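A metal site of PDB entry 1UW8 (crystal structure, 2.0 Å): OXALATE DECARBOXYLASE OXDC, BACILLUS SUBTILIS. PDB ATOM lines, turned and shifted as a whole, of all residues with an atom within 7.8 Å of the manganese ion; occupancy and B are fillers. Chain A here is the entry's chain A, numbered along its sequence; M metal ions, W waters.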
ATOM      1  N   VAL A 262       7.320   0.861  21.512  1.00  0.00           N
ATOM      2  CA  VAL A 262       6.527   0.835  22.710  1.00  0.00           C
ATOM      3  C   VAL A 262       5.813  -0.515  22.850  1.00  0.00           C
ATOM      4  O   VAL A 262       5.177  -0.997  21.902  1.00  0.00           O
ATOM      5  CB  VAL A 262       5.473   1.943  22.691  1.00  0.00           C
ATOM      6  CG1 VAL A 262       4.675   1.947  24.003  1.00  0.00           C
ATOM      7  CG2 VAL A 262       6.121   3.328  22.392  1.00  0.00           C
ATOM      8  N   ARG A 270      -0.295   3.532  26.984  1.00  0.00           N
ATOM      9  CA  ARG A 270       0.611   4.649  26.788  1.00  0.00           C
ATOM     10  C   ARG A 270      -0.145   5.860  27.311  1.00  0.00           C
ATOM     11  O   ARG A 270      -1.238   6.179  26.845  1.00  0.00           O
ATOM     12  CB  ARG A 270       0.986   4.806  25.313  1.00  0.00           C
ATOM     13  CG  ARG A 270       1.935   5.953  24.994  1.00  0.00           C
ATOM     14  CD  ARG A 270       3.410   5.611  25.140  1.00  0.00           C
ATOM     15  NE  ARG A 270       4.244   6.737  24.770  1.00  0.00           N
ATOM     16  CZ  ARG A 270       4.424   7.837  25.545  1.00  0.00           C
ATOM     17  NH1 ARG A 270       3.890   7.937  26.763  1.00  0.00           N
ATOM     18  NH2 ARG A 270       5.161   8.821  25.085  1.00  0.00           N
ATOM     19  N   GLU A 271       0.430   6.518  28.316  1.00  0.00           N
ATOM     20  CA  GLU A 271      -0.242   7.559  29.075  1.00  0.00           C
ATOM     21  C   GLU A 271      -0.622   8.784  28.220  1.00  0.00           C
ATOM     22  O   GLU A 271      -0.159   8.956  27.103  1.00  0.00           O
ATOM     23  CB  GLU A 271       0.619   8.009  30.288  1.00  0.00           C
ATOM     24  CG  GLU A 271       1.856   8.800  29.916  1.00  0.00           C
ATOM     25  CD  GLU A 271       2.515   9.525  31.072  1.00  0.00           C
ATOM     26  OE1 GLU A 271       1.915   9.615  32.158  1.00  0.00           O
ATOM     27  OE2 GLU A 271       3.658  10.025  30.889  1.00  0.00           O
ATOM     28  N   HIS A 273      -0.253  12.153  26.848  1.00  0.00           N
ATOM     29  CA  HIS A 273       0.936  12.945  26.525  1.00  0.00           C
ATOM     30  C   HIS A 273       0.761  13.711  25.206  1.00  0.00           C
ATOM     31  O   HIS A 273      -0.223  13.504  24.466  1.00  0.00           O
ATOM     32  CB  HIS A 273       2.196  12.060  26.497  1.00  0.00           C
ATOM     33  CG  HIS A 273       2.247  11.121  25.328  1.00  0.00           C
ATOM     34  ND1 HIS A 273       1.397  10.045  25.216  1.00  0.00           N
ATOM     35  CD2 HIS A 273       3.028  11.107  24.225  1.00  0.00           C
ATOM     36  CE1 HIS A 273       1.641   9.406  24.079  1.00  0.00           C
ATOM     37  NE2 HIS A 273       2.612  10.049  23.456  1.00  0.00           N
ATOM     38  N   TRP A 274       1.719  14.570  24.902  1.00  0.00           N
ATOM     39  CA  TRP A 274       1.868  15.062  23.546  1.00  0.00           C
ATOM     40  C   TRP A 274       3.352  15.207  23.238  1.00  0.00           C
ATOM     41  O   TRP A 274       4.205  15.006  24.117  1.00  0.00           O
ATOM     42  CB  TRP A 274       1.129  16.404  23.333  1.00  0.00           C
ATOM     43  CG  TRP A 274       1.706  17.616  23.973  1.00  0.00           C
ATOM     44  CD1 TRP A 274       2.598  18.496  23.438  1.00  0.00           C
ATOM     45  CD2 TRP A 274       1.396  18.115  25.281  1.00  0.00           C
ATOM     46  NE1 TRP A 274       2.873  19.512  24.326  1.00  0.00           N
ATOM     47  CE2 TRP A 274       2.141  19.310  25.468  1.00  0.00           C
ATOM     48  CE3 TRP A 274       0.565  17.678  26.320  1.00  0.00           C
ATOM     49  CZ2 TRP A 274       2.059  20.058  26.635  1.00  0.00           C
ATOM     50  CZ3 TRP A 274       0.491  18.431  27.477  1.00  0.00           C
ATOM     51  CH2 TRP A 274       1.240  19.610  27.622  1.00  0.00           C
ATOM     52  N   HIS A 275       3.660  15.531  21.981  1.00  0.00           N
ATOM     53  CA  HIS A 275       5.008  15.794  21.552  1.00  0.00           C
ATOM     54  C   HIS A 275       5.134  17.244  21.159  1.00  0.00           C
ATOM     55  O   HIS A 275       4.350  17.733  20.345  1.00  0.00           O
ATOM     56  CB  HIS A 275       5.344  14.866  20.420  1.00  0.00           C
ATOM     57  CG  HIS A 275       5.165  13.426  20.785  1.00  0.00           C
ATOM     58  ND1 HIS A 275       6.142  12.706  21.422  1.00  0.00           N
ATOM     59  CD2 HIS A 275       4.084  12.622  20.705  1.00  0.00           C
ATOM     60  CE1 HIS A 275       5.689  11.494  21.683  1.00  0.00           C
ATOM     61  NE2 HIS A 275       4.440  11.412  21.254  1.00  0.00           N
ATOM     62  N   GLU A 280       3.666  12.782  15.048  1.00  0.00           N
ATOM     63  CA  GLU A 280       3.918  11.360  15.235  1.00  0.00           C
ATOM     64  C   GLU A 280       3.282  10.523  14.134  1.00  0.00           C
ATOM     65  O   GLU A 280       2.096  10.654  13.837  1.00  0.00           O
ATOM     66  CB  GLU A 280       3.330  10.870  16.563  1.00  0.00           C
ATOM     67  CG  GLU A 280       3.569   9.397  16.879  1.00  0.00           C
ATOM     68  CD  GLU A 280       3.112   9.020  18.282  1.00  0.00           C
ATOM     69  OE1 GLU A 280       3.327   9.846  19.175  1.00  0.00           O
ATOM     70  OE2 GLU A 280       2.555   7.938  18.518  1.00  0.00           O
ATOM     71  N   TRP A 281       4.082   9.642  13.581  1.00  0.00           N
ATOM     72  CA  TRP A 281       3.654   8.616  12.663  1.00  0.00           C
ATOM     73  C   TRP A 281       3.812   7.290  13.416  1.00  0.00           C
ATOM     74  O   TRP A 281       4.803   7.093  14.158  1.00  0.00           O
ATOM     75  CB  TRP A 281       4.532   8.675  11.422  1.00  0.00           C
ATOM     76  CG  TRP A 281       4.163   7.735  10.333  1.00  0.00           C
ATOM     77  CD1 TRP A 281       3.460   8.020   9.210  1.00  0.00           C
ATOM     78  CD2 TRP A 281       4.510   6.349  10.242  1.00  0.00           C
ATOM     79  NE1 TRP A 281       3.357   6.908   8.414  1.00  0.00           N
ATOM     80  CE2 TRP A 281       3.978   5.862   9.031  1.00  0.00           C
ATOM     81  CE3 TRP A 281       5.238   5.469  11.061  1.00  0.00           C
ATOM     82  CZ2 TRP A 281       4.122   4.520   8.630  1.00  0.00           C
ATOM     83  CZ3 TRP A 281       5.370   4.154  10.662  1.00  0.00           C
ATOM     84  CH2 TRP A 281       4.813   3.699   9.456  1.00  0.00           C
ATOM     85  N   GLN A 282       2.816   6.413  13.276  1.00  0.00           N
ATOM     86  CA  GLN A 282       2.725   5.163  14.057  1.00  0.00           C
ATOM     87  C   GLN A 282       2.621   3.963  13.165  1.00  0.00           C
ATOM     88  O   GLN A 282       1.962   4.026  12.121  1.00  0.00           O
ATOM     89  CB  GLN A 282       1.461   5.149  14.932  1.00  0.00           C
ATOM     90  CG  GLN A 282       1.265   6.346  15.826  1.00  0.00           C
ATOM     91  CD  GLN A 282      -0.022   6.237  16.634  1.00  0.00           C
ATOM     92  OE1 GLN A 282      -1.012   5.666  16.157  1.00  0.00           O
ATOM     93  NE2 GLN A 282      -0.011   6.780  17.850  1.00  0.00           N
ATOM     94  N   MET A 291      -6.935   4.976  20.291  1.00  0.00           N
ATOM     95  CA  MET A 291      -6.336   6.257  20.638  1.00  0.00           C
ATOM     96  C   MET A 291      -7.323   7.361  20.357  1.00  0.00           C
ATOM     97  O   MET A 291      -7.891   7.393  19.286  1.00  0.00           O
ATOM     98  CB  MET A 291      -5.111   6.503  19.747  1.00  0.00           C
ATOM     99  CG  MET A 291      -4.625   7.919  19.724  1.00  0.00           C
ATOM    100  SD  MET A 291      -3.009   8.147  18.892  1.00  0.00           S
ATOM    101  CE  MET A 291      -3.509   7.910  17.181  1.00  0.00           C
ATOM    102  N   VAL A 313      -0.460  11.301  14.581  1.00  0.00           N
ATOM    103  CA  VAL A 313      -0.869  12.334  15.522  1.00  0.00           C
ATOM    104  C   VAL A 313      -0.193  13.629  15.121  1.00  0.00           C
ATOM    105  O   VAL A 313       1.005  13.785  15.324  1.00  0.00           O
ATOM    106  CB  VAL A 313      -0.456  12.030  16.970  1.00  0.00           C
ATOM    107  CG1 VAL A 313      -1.052  13.064  17.946  1.00  0.00           C
ATOM    108  CG2 VAL A 313      -0.837  10.598  17.409  1.00  0.00           C
ATOM    109  N   MET A 317      -0.785  17.480  19.255  1.00  0.00           N
ATOM    110  CA  MET A 317      -2.110  17.039  19.643  1.00  0.00           C
ATOM    111  C   MET A 317      -2.032  16.035  20.822  1.00  0.00           C
ATOM    112  O   MET A 317      -1.134  15.212  20.890  1.00  0.00           O
ATOM    113  CB  MET A 317      -2.858  16.429  18.439  1.00  0.00           C
ATOM    114  CG  MET A 317      -3.219  17.475  17.381  1.00  0.00           C
ATOM    115  SD  MET A 317      -4.434  16.887  16.240  1.00  0.00           S
ATOM    116  CE  MET A 317      -4.673  18.371  15.247  1.00  0.00           C
ATOM    117  N   GLY A 318      -2.972  16.146  21.747  1.00  0.00           N
ATOM    118  CA  GLY A 318      -2.994  15.314  22.933  1.00  0.00           C
ATOM    119  C   GLY A 318      -3.434  13.927  22.541  1.00  0.00           C
ATOM    120  O   GLY A 318      -4.293  13.759  21.687  1.00  0.00           O
ATOM    121  N   HIS A 319      -2.855  12.917  23.189  1.00  0.00           N
ATOM    122  CA  HIS A 319      -3.239  11.555  22.927  1.00  0.00           C
ATOM    123  C   HIS A 319      -2.780  10.549  23.976  1.00  0.00           C
ATOM    124  O   HIS A 319      -2.059  10.883  24.907  1.00  0.00           O
ATOM    125  CB  HIS A 319      -2.725  11.128  21.554  1.00  0.00           C
ATOM    126  CG  HIS A 319      -1.247  11.234  21.385  1.00  0.00           C
ATOM    127  ND1 HIS A 319      -0.595  12.423  21.137  1.00  0.00           N
ATOM    128  CD2 HIS A 319      -0.288  10.283  21.436  1.00  0.00           C
ATOM    129  CE1 HIS A 319       0.701  12.180  20.998  1.00  0.00           C
ATOM    130  NE2 HIS A 319       0.912  10.891  21.174  1.00  0.00           N
ATOM    131  N   TYR A 320      -3.347   9.351  23.869  1.00  0.00           N
ATOM    132  CA  TYR A 320      -2.970   8.175  24.667  1.00  0.00           C
ATOM    133  C   TYR A 320      -3.108   6.972  23.701  1.00  0.00           C
ATOM    134  O   TYR A 320      -3.773   7.075  22.670  1.00  0.00           O
ATOM    135  CB  TYR A 320      -3.895   7.974  25.867  1.00  0.00           C
ATOM    136  CG  TYR A 320      -5.295   7.662  25.459  1.00  0.00           C
ATOM    137  CD1 TYR A 320      -5.736   6.351  25.316  1.00  0.00           C
ATOM    138  CD2 TYR A 320      -6.193   8.680  25.181  1.00  0.00           C
ATOM    139  CE1 TYR A 320      -7.043   6.071  24.871  1.00  0.00           C
ATOM    140  CE2 TYR A 320      -7.483   8.415  24.765  1.00  0.00           C
ATOM    141  CZ  TYR A 320      -7.908   7.113  24.602  1.00  0.00           C
ATOM    142  OH  TYR A 320      -9.200   6.851  24.156  1.00  0.00           O
ATOM    143  N   VAL A 321      -2.499   5.843  24.036  1.00  0.00           N
ATOM    144  CA  VAL A 321      -2.735   4.621  23.269  1.00  0.00           C
ATOM    145  C   VAL A 321      -3.031   3.491  24.245  1.00  0.00           C
ATOM    146  O   VAL A 321      -2.149   3.040  24.981  1.00  0.00           O
ATOM    147  CB  VAL A 321      -1.546   4.283  22.363  1.00  0.00           C
ATOM    148  CG1 VAL A 321      -1.918   3.184  21.392  1.00  0.00           C
ATOM    149  CG2 VAL A 321      -1.074   5.508  21.584  1.00  0.00           C
ATOM    150  N   PHE A 331       3.889  -1.132  19.226  1.00  0.00           N
ATOM    151  CA  PHE A 331       3.865  -0.173  18.136  1.00  0.00           C
ATOM    152  C   PHE A 331       5.076   0.742  18.157  1.00  0.00           C
ATOM    153  O   PHE A 331       5.813   0.853  19.136  1.00  0.00           O
ATOM    154  CB  PHE A 331       2.559   0.657  18.151  1.00  0.00           C
ATOM    155  CG  PHE A 331       2.410   1.568  19.365  1.00  0.00           C
ATOM    156  CD1 PHE A 331       2.776   2.909  19.292  1.00  0.00           C
ATOM    157  CD2 PHE A 331       1.857   1.093  20.547  1.00  0.00           C
ATOM    158  CE1 PHE A 331       2.614   3.748  20.379  1.00  0.00           C
ATOM    159  CE2 PHE A 331       1.684   1.935  21.665  1.00  0.00           C
ATOM    160  CZ  PHE A 331       2.094   3.256  21.579  1.00  0.00           C
ATOM    161  N   GLU A 333       6.467   4.694  17.424  1.00  0.00           N
ATOM    162  CA  GLU A 333       6.274   6.128  17.363  1.00  0.00           C
ATOM    163  C   GLU A 333       7.461   6.685  16.585  1.00  0.00           C
ATOM    164  O   GLU A 333       8.621   6.538  17.036  1.00  0.00           O
ATOM    165  CB  GLU A 333       6.289   6.758  18.772  1.00  0.00           C
ATOM    166  CG  GLU A 333       5.249   6.239  19.746  1.00  0.00           C
ATOM    167  CD  GLU A 333       5.490   6.697  21.180  1.00  0.00           C
ATOM    168  OE1 GLU A 333       6.654   6.985  21.566  1.00  0.00           O
ATOM    169  OE2 GLU A 333       4.491   6.749  21.939  1.00  0.00           O
ATOM    170  N   ILE A 334       7.185   7.300  15.435  1.00  0.00           N
ATOM    171  CA  ILE A 334       8.201   7.852  14.533  1.00  0.00           C
ATOM    172  C   ILE A 334       8.004   9.369  14.353  1.00  0.00           C
ATOM    173  O   ILE A 334       6.876   9.863  14.230  1.00  0.00           O
ATOM    174  CB  ILE A 334       8.112   7.144  13.146  1.00  0.00           C
ATOM    175  CG1 ILE A 334       8.186   5.632  13.308  1.00  0.00           C
ATOM    176  CG2 ILE A 334       9.211   7.620  12.238  1.00  0.00           C
ATOM    177  CD1 ILE A 334       9.520   5.118  13.877  1.00  0.00           C
ATOM    178  N   PHE A 335       9.120  10.105  14.308  1.00  0.00           N
ATOM    179  CA  PHE A 335       9.110  11.570  14.204  1.00  0.00           C
ATOM    180  C   PHE A 335      10.158  12.035  13.213  1.00  0.00           C
ATOM    181  O   PHE A 335      11.266  11.508  13.222  1.00  0.00           O
ATOM    182  CB  PHE A 335       9.410  12.216  15.567  1.00  0.00           C
ATOM    183  CG  PHE A 335       8.522  11.723  16.642  1.00  0.00           C
ATOM    184  CD1 PHE A 335       7.354  12.401  16.973  1.00  0.00           C
ATOM    185  CD2 PHE A 335       8.828  10.545  17.298  1.00  0.00           C
ATOM    186  CE1 PHE A 335       6.505  11.896  17.959  1.00  0.00           C
ATOM    187  CE2 PHE A 335       7.979  10.046  18.268  1.00  0.00           C
ATOM    188  CZ  PHE A 335       6.831  10.737  18.592  1.00  0.00           C
ATOM    189  N   TYR A 340      13.645  12.752  20.082  1.00  0.00           N
ATOM    190  CA  TYR A 340      12.383  12.338  20.644  1.00  0.00           C
ATOM    191  C   TYR A 340      12.116  13.243  21.849  1.00  0.00           C
ATOM    192  O   TYR A 340      13.019  13.479  22.653  1.00  0.00           O
ATOM    193  CB  TYR A 340      12.502  10.899  21.128  1.00  0.00           C
ATOM    194  CG  TYR A 340      11.226  10.349  21.707  1.00  0.00           C
ATOM    195  CD1 TYR A 340      10.365   9.580  20.923  1.00  0.00           C
ATOM    196  CD2 TYR A 340      10.888  10.562  23.030  1.00  0.00           C
ATOM    197  CE1 TYR A 340       9.189   9.068  21.454  1.00  0.00           C
ATOM    198  CE2 TYR A 340       9.724  10.057  23.564  1.00  0.00           C
ATOM    199  CZ  TYR A 340       8.882   9.301  22.773  1.00  0.00           C
ATOM    200  OH  TYR A 340       7.725   8.779  23.294  1.00  0.00           O
ATOM    201  N   ALA A 341      10.886  13.735  21.967  1.00  0.00           N
ATOM    202  CA  ALA A 341      10.492  14.502  23.155  1.00  0.00           C
ATOM    203  C   ALA A 341       9.016  14.274  23.424  1.00  0.00           C
ATOM    204  O   ALA A 341       8.201  14.183  22.486  1.00  0.00           O
ATOM    205  CB  ALA A 341      10.742  15.985  22.920  1.00  0.00           C
ATOM    206  N   ASP A 342       8.666  14.126  24.696  1.00  0.00           N
ATOM    207  CA  ASP A 342       7.267  14.134  25.079  1.00  0.00           C
ATOM    208  C   ASP A 342       7.019  14.954  26.347  1.00  0.00           C
ATOM    209  O   ASP A 342       7.937  15.213  27.134  1.00  0.00           O
ATOM    210  CB  ASP A 342       6.673  12.704  25.145  1.00  0.00           C
ATOM    211  CG  ASP A 342       7.265  11.798  26.264  1.00  0.00           C
ATOM    212  OD1 ASP A 342       8.353  12.072  26.821  1.00  0.00           O
ATOM    213  OD2 ASP A 342       6.705  10.732  26.608  1.00  0.00           O
HETATM  214 MN    MN M   1       2.914   9.867  21.218  1.00  0.00          MN
HETATM  215  O   HOH W   1       2.311   7.797  21.105  1.00  0.00           O
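Residues that only touch the manganese ion: Glu 333 (3.6 Å). Of the 23 residues printed, 5 come within 4 Å of the manganese ion.
N of Val 313 is in hydrogen-bond range of O of Glu 280, 2.7 Å away. The side-chain hydroxyl (OH) of Tyr 340 lies within hydrogen-bond range of the side-chain carboxylate (OE1) of Glu 333, at 2.7 Å. OE2 of Glu 280 sits at hydrogen-bond distance from NE2 of Gln 282 (2.9 Å). The backbone carbonyl oxygen (O) of Met 317 is in hydrogen-bond range of a ring nitrogen (ND1) of His 319 (2.9 Å). The guanidinium group (NH2) of Arg 270 lies close to a ring nitrogen (NE2) of His 273. ND1 of His 275 sits at hydrogen-bond distance from O of Ala 341 (2.7 Å). A ring nitrogen (ND1) of His 273 is in hydrogen-bond range of the backbone carbonyl oxygen (O) of Glu 271 (2.7 Å). OE2 of Glu 333 lies within salt-bridge range of NE of Arg 270, 2.8 Å away.
OE1 of Glu 280 is bound to the manganese ion, at 2.1 Å. The manganese ion is bound by water W1 (2.2 Å). A ring nitrogen (NE2) of His 275 is bound to the manganese ion. A ring nitrogen (NE2) of His 319 binds the manganese ion (2.2 Å). NE2 of His 273 is bound to the manganese ion (2.3 Å).
Water W1 lies within hydrogen-bond range of OE2 of Glu 333 (2.6 Å) and OE2 of Glu 280 (2.6 Å).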
